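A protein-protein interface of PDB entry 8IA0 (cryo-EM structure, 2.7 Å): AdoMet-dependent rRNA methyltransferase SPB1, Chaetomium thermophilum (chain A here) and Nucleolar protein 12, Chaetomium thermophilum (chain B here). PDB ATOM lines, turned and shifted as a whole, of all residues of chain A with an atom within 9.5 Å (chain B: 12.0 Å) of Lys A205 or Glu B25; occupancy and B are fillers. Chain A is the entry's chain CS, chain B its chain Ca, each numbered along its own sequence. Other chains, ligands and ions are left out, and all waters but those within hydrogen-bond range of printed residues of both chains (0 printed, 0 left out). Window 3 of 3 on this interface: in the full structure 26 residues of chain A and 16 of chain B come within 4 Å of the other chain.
O of Leu A175 lies within hydrogen-bond range of N of Lys A202 (3.4 Å).
The side-chain carboxylate (OD2) of Asp A208 sits at hydrogen-bond distance from the backbone NH (N) of Phe B28 (3.2 Å).
Among the printed residues, pairs that only touch across the chains: Arg A206 with Glu B25, Gln A174 with Ile B26, Arg A206 with Ile B26, Leu A175 with Ile B26, Leu A211 with Phe B28, Pro A204 with Ile B26, Lys A205 with Glu B25 and Pro A204 with Glu B25.
Hydrophobic or aromatic side chains of chain B within 4 Å of the printed part of chain A: Ile B26 and Phe B28. Of the 13 printed residues of chain A, 7 touch a printed residue of chain B. Hydrophobic or aromatic side chains of chain A that line the printed part of chain B: Leu A175 and Pro A204. Among the printed residues, 9 pairs touch across the chains. Among the printed residues, no Asp or Glu carboxylate lies within 4 Å of a Lys or Arg side-chain nitrogen of the other chain.
Lys A205 touches just one residue of chain B: Glu B25 (3.9 Å). No residue of chain B comes within 4 Å of Ala A203. Of chain B, only Glu B25 (3.9 Å) and Ile B26 (3.7 Å) come within 4 Å of Pro A204. Of chain B, only Glu B25 and Ile B26 come within 4 Å of Arg A206. Printed residues of chain B within 4 Å of Gln A174: Ile B26 (3.3 Å). Printed residues of chain B within 4 Å of Leu A211: Phe B28. Printed residues of chain A within 4 Å of Phe B28: Asp A208 (3.2 Å) and Leu A211 (3.7 Å). Thr B27 touches none of the printed residues of chain A. Asp B29 touches none of the printed residues of chain A. The nearest residue of chain A that does not touch Glu B25 is Ala A203 (5.8 Å). The nearest printed residue of chain B that does not touch Asp A208 is Thr B27 (4.1 Å).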
ATOM      1  N   THR A 146      13.062   0.974   0.061  1.00  0.00           N
ATOM      2  CA  THR A 146      12.988   1.951   1.141  1.00  0.00           C
ATOM      3  C   THR A 146      12.285   1.370   2.359  1.00  0.00           C
ATOM      4  O   THR A 146      12.551   1.777   3.496  1.00  0.00           O
ATOM      5  CB  THR A 146      12.265   3.209   0.663  1.00  0.00           C
ATOM      6  OG1 THR A 146      11.004   2.843   0.088  1.00  0.00           O
ATOM      7  CG2 THR A 146      13.094   3.926  -0.383  1.00  0.00           C
ATOM      8  N   GLU A 147      11.374   0.421   2.140  1.00  0.00           N
ATOM      9  CA  GLU A 147      10.683  -0.210   3.256  1.00  0.00           C
ATOM     10  C   GLU A 147      11.590  -1.202   3.972  1.00  0.00           C
ATOM     11  O   GLU A 147      11.471  -1.397   5.187  1.00  0.00           O
ATOM     12  CB  GLU A 147       9.410  -0.901   2.760  1.00  0.00           C
ATOM     13  CG  GLU A 147       8.471  -1.494   3.831  1.00  0.00           C
ATOM     14  CD  GLU A 147       8.341  -0.680   5.121  1.00  0.00           C
ATOM     15  OE1 GLU A 147       8.548   0.554   5.116  1.00  0.00           O
ATOM     16  OE2 GLU A 147       8.022  -1.294   6.160  1.00  0.00           O
ATOM     17  N   GLN A 174      17.914  12.130  -4.466  1.00  0.00           N
ATOM     18  CA  GLN A 174      17.295  12.661  -3.260  1.00  0.00           C
ATOM     19  C   GLN A 174      17.096  11.604  -2.184  1.00  0.00           C
ATOM     20  O   GLN A 174      16.763  11.956  -1.048  1.00  0.00           O
ATOM     21  CB  GLN A 174      15.947  13.302  -3.594  1.00  0.00           C
ATOM     22  CG  GLN A 174      15.967  14.193  -4.819  1.00  0.00           C
ATOM     23  CD  GLN A 174      16.699  15.495  -4.579  1.00  0.00           C
ATOM     24  OE1 GLN A 174      16.324  16.277  -3.706  1.00  0.00           O
ATOM     25  NE2 GLN A 174      17.749  15.736  -5.354  1.00  0.00           N
ATOM     26  N   LEU A 175      17.290  10.326  -2.509  1.00  0.00           N
ATOM     27  CA  LEU A 175      17.085   9.248  -1.554  1.00  0.00           C
ATOM     28  C   LEU A 175      18.369   8.543  -1.147  1.00  0.00           C
ATOM     29  O   LEU A 175      18.383   7.875  -0.109  1.00  0.00           O
ATOM     30  CB  LEU A 175      16.109   8.213  -2.129  1.00  0.00           C
ATOM     31  CG  LEU A 175      14.943   7.821  -1.224  1.00  0.00           C
ATOM     32  CD1 LEU A 175      14.347   9.057  -0.586  1.00  0.00           C
ATOM     33  CD2 LEU A 175      13.888   7.077  -2.018  1.00  0.00           C
ATOM     34  N   PHE A 201      21.923   5.243   1.683  1.00  0.00           N
ATOM     35  CA  PHE A 201      20.506   5.545   1.839  1.00  0.00           C
ATOM     36  C   PHE A 201      20.308   6.344   3.120  1.00  0.00           C
ATOM     37  O   PHE A 201      20.714   5.906   4.200  1.00  0.00           O
ATOM     38  CB  PHE A 201      19.710   4.239   1.814  1.00  0.00           C
ATOM     39  CG  PHE A 201      18.274   4.352   2.234  1.00  0.00           C
ATOM     40  CD1 PHE A 201      17.907   4.493   3.561  1.00  0.00           C
ATOM     41  CD2 PHE A 201      17.279   4.165   1.283  1.00  0.00           C
ATOM     42  CE1 PHE A 201      16.568   4.544   3.909  1.00  0.00           C
ATOM     43  CE2 PHE A 201      15.952   4.221   1.622  1.00  0.00           C
ATOM     44  CZ  PHE A 201      15.596   4.406   2.936  1.00  0.00           C
ATOM     45  N   LYS A 202      19.660   7.504   3.001  1.00  0.00           N
ATOM     46  CA  LYS A 202      19.737   8.512   4.053  1.00  0.00           C
ATOM     47  C   LYS A 202      18.951   8.128   5.300  1.00  0.00           C
ATOM     48  O   LYS A 202      19.198   8.690   6.372  1.00  0.00           O
ATOM     49  CB  LYS A 202      19.255   9.857   3.513  1.00  0.00           C
ATOM     50  CG  LYS A 202      20.331  10.644   2.811  1.00  0.00           C
ATOM     51  CD  LYS A 202      19.747  11.363   1.609  1.00  0.00           C
ATOM     52  CE  LYS A 202      20.822  11.982   0.744  1.00  0.00           C
ATOM     53  NZ  LYS A 202      20.324  13.233   0.120  1.00  0.00           N
ATOM     54  N   ALA A 203      17.994   7.212   5.183  1.00  0.00           N
ATOM     55  CA  ALA A 203      17.127   6.818   6.288  1.00  0.00           C
ATOM     56  C   ALA A 203      16.411   8.024   6.880  1.00  0.00           C
ATOM     57  O   ALA A 203      16.786   8.489   7.961  1.00  0.00           O
ATOM     58  CB  ALA A 203      17.930   6.087   7.366  1.00  0.00           C
ATOM     59  N   PRO A 204      15.416   8.582   6.195  1.00  0.00           N
ATOM     60  CA  PRO A 204      14.572   9.607   6.817  1.00  0.00           C
ATOM     61  C   PRO A 204      13.529   8.976   7.724  1.00  0.00           C
ATOM     62  O   PRO A 204      13.216   7.788   7.636  1.00  0.00           O
ATOM     63  CB  PRO A 204      13.907  10.310   5.624  1.00  0.00           C
ATOM     64  CG  PRO A 204      14.524   9.668   4.376  1.00  0.00           C
ATOM     65  CD  PRO A 204      15.040   8.340   4.795  1.00  0.00           C
ATOM     66  N   LYS A 205      12.978   9.807   8.610  1.00  0.00           N
ATOM     67  CA  LYS A 205      11.917   9.333   9.492  1.00  0.00           C
ATOM     68  C   LYS A 205      10.673   8.953   8.702  1.00  0.00           C
ATOM     69  O   LYS A 205      10.026   7.942   8.996  1.00  0.00           O
ATOM     70  CB  LYS A 205      11.583  10.393  10.540  1.00  0.00           C
ATOM     71  CG  LYS A 205      12.737  10.729  11.468  1.00  0.00           C
ATOM     72  CD  LYS A 205      12.345  11.779  12.496  1.00  0.00           C
ATOM     73  CE  LYS A 205      12.105  13.126  11.835  1.00  0.00           C
ATOM     74  NZ  LYS A 205      13.335  13.683  11.211  1.00  0.00           N
ATOM     75  N   ARG A 206      10.317   9.756   7.704  1.00  0.00           N
ATOM     76  CA  ARG A 206       9.199   9.454   6.824  1.00  0.00           C
ATOM     77  C   ARG A 206       9.502  10.041   5.454  1.00  0.00           C
ATOM     78  O   ARG A 206      10.112  11.107   5.350  1.00  0.00           O
ATOM     79  CB  ARG A 206       7.857   9.996   7.350  1.00  0.00           C
ATOM     80  CG  ARG A 206       7.671  11.515   7.314  1.00  0.00           C
ATOM     81  CD  ARG A 206       8.661  12.249   8.203  1.00  0.00           C
ATOM     82  NE  ARG A 206       8.946  13.593   7.720  1.00  0.00           N
ATOM     83  CZ  ARG A 206       9.945  13.891   6.903  1.00  0.00           C
ATOM     84  NH1 ARG A 206      10.767  12.960   6.450  1.00  0.00           N
ATOM     85  NH2 ARG A 206      10.128  15.156   6.534  1.00  0.00           N
ATOM     86  N   ILE A 207       9.085   9.333   4.410  1.00  0.00           N
ATOM     87  CA  ILE A 207       9.374   9.710   3.032  1.00  0.00           C
ATOM     88  C   ILE A 207       8.091  10.219   2.395  1.00  0.00           C
ATOM     89  O   ILE A 207       7.020   9.626   2.575  1.00  0.00           O
ATOM     90  CB  ILE A 207       9.962   8.522   2.243  1.00  0.00           C
ATOM     91  CG1 ILE A 207      11.485   8.506   2.366  1.00  0.00           C
ATOM     92  CG2 ILE A 207       9.550   8.575   0.774  1.00  0.00           C
ATOM     93  CD1 ILE A 207      12.132   7.312   1.700  1.00  0.00           C
ATOM     94  N   ASP A 208       8.197  11.322   1.668  1.00  0.00           N
ATOM     95  CA  ASP A 208       7.042  11.909   1.001  1.00  0.00           C
ATOM     96  C   ASP A 208       6.445  10.906   0.020  1.00  0.00           C
ATOM     97  O   ASP A 208       7.162  10.423  -0.866  1.00  0.00           O
ATOM     98  CB  ASP A 208       7.461  13.183   0.277  1.00  0.00           C
ATOM     99  CG  ASP A 208       6.284  14.049  -0.118  1.00  0.00           C
ATOM    100  OD1 ASP A 208       5.144  13.732   0.274  1.00  0.00           O
ATOM    101  OD2 ASP A 208       6.503  15.057  -0.821  1.00  0.00           O
ATOM    102  N   LEU A 211       7.105  11.450  -3.553  1.00  0.00           N
ATOM    103  CA  LEU A 211       8.428  11.099  -4.055  1.00  0.00           C
ATOM    104  C   LEU A 211       8.475   9.664  -4.562  1.00  0.00           C
ATOM    105  O   LEU A 211       9.303   9.337  -5.418  1.00  0.00           O
ATOM    106  CB  LEU A 211       9.475  11.317  -2.962  1.00  0.00           C
ATOM    107  CG  LEU A 211      10.949  11.337  -3.369  1.00  0.00           C
ATOM    108  CD1 LEU A 211      11.122  11.905  -4.768  1.00  0.00           C
ATOM    109  CD2 LEU A 211      11.768  12.131  -2.363  1.00  0.00           C
ATOM    110  N   GLU B  25      14.668  13.842   7.038  1.00  0.00           N
ATOM    111  CA  GLU B  25      13.492  14.674   6.821  1.00  0.00           C
ATOM    112  C   GLU B  25      13.554  15.368   5.466  1.00  0.00           C
ATOM    113  O   GLU B  25      14.011  16.505   5.363  1.00  0.00           O
ATOM    114  CB  GLU B  25      13.354  15.711   7.938  1.00  0.00           C
ATOM    115  N   ILE B  26      13.092  14.677   4.425  1.00  0.00           N
ATOM    116  CA  ILE B  26      13.133  15.182   3.059  1.00  0.00           C
ATOM    117  C   ILE B  26      11.731  15.134   2.470  1.00  0.00           C
ATOM    118  O   ILE B  26      10.905  14.304   2.866  1.00  0.00           O
ATOM    119  CB  ILE B  26      14.123  14.384   2.184  1.00  0.00           C
ATOM    120  CG1 ILE B  26      13.577  12.985   1.895  1.00  0.00           C
ATOM    121  CG2 ILE B  26      15.493  14.316   2.847  1.00  0.00           C
ATOM    122  CD1 ILE B  26      14.632  12.000   1.461  1.00  0.00           C
ATOM    123  N   THR B  27      11.464  16.034   1.530  1.00  0.00           N
ATOM    124  CA  THR B  27      10.174  16.158   0.868  1.00  0.00           C
ATOM    125  C   THR B  27      10.378  16.255  -0.642  1.00  0.00           C
ATOM    126  O   THR B  27      11.479  16.056  -1.159  1.00  0.00           O
ATOM    127  CB  THR B  27       9.406  17.379   1.385  1.00  0.00           C
ATOM    128  OG1 THR B  27      10.232  18.544   1.282  1.00  0.00           O
ATOM    129  CG2 THR B  27       8.992  17.179   2.836  1.00  0.00           C
ATOM    130  N   PHE B  28       9.294  16.568  -1.347  1.00  0.00           N
ATOM    131  CA  PHE B  28       9.334  16.730  -2.796  1.00  0.00           C
ATOM    132  C   PHE B  28       9.817  18.137  -3.123  1.00  0.00           C
ATOM    133  O   PHE B  28       9.118  19.120  -2.854  1.00  0.00           O
ATOM    134  CB  PHE B  28       7.956  16.471  -3.398  1.00  0.00           C
ATOM    135  CG  PHE B  28       7.993  16.053  -4.839  1.00  0.00           C
ATOM    136  CD1 PHE B  28       8.189  16.986  -5.841  1.00  0.00           C
ATOM    137  CD2 PHE B  28       7.827  14.727  -5.191  1.00  0.00           C
ATOM    138  CE1 PHE B  28       8.222  16.605  -7.166  1.00  0.00           C
ATOM    139  CE2 PHE B  28       7.859  14.340  -6.515  1.00  0.00           C
ATOM    140  CZ  PHE B  28       8.056  15.279  -7.503  1.00  0.00           C
ATOM    141  N   ASP B  29      11.008  18.238  -3.704  1.00  0.00           N
ATOM    142  CA  ASP B  29      11.583  19.518  -4.112  1.00  0.00           C
ATOM    143  C   ASP B  29      11.239  19.722  -5.584  1.00  0.00           C
ATOM    144  O   ASP B  29      11.946  19.256  -6.477  1.00  0.00           O
ATOM    145  CB  ASP B  29      13.088  19.543  -3.870  1.00  0.00           C
ATOM    146  CG  ASP B  29      13.450  20.117  -2.514  1.00  0.00           C
ATOM    147  OD1 ASP B  29      12.542  20.614  -1.815  1.00  0.00           O
ATOM    148  OD2 ASP B  29      14.642  20.070  -2.146  1.00  0.00           O
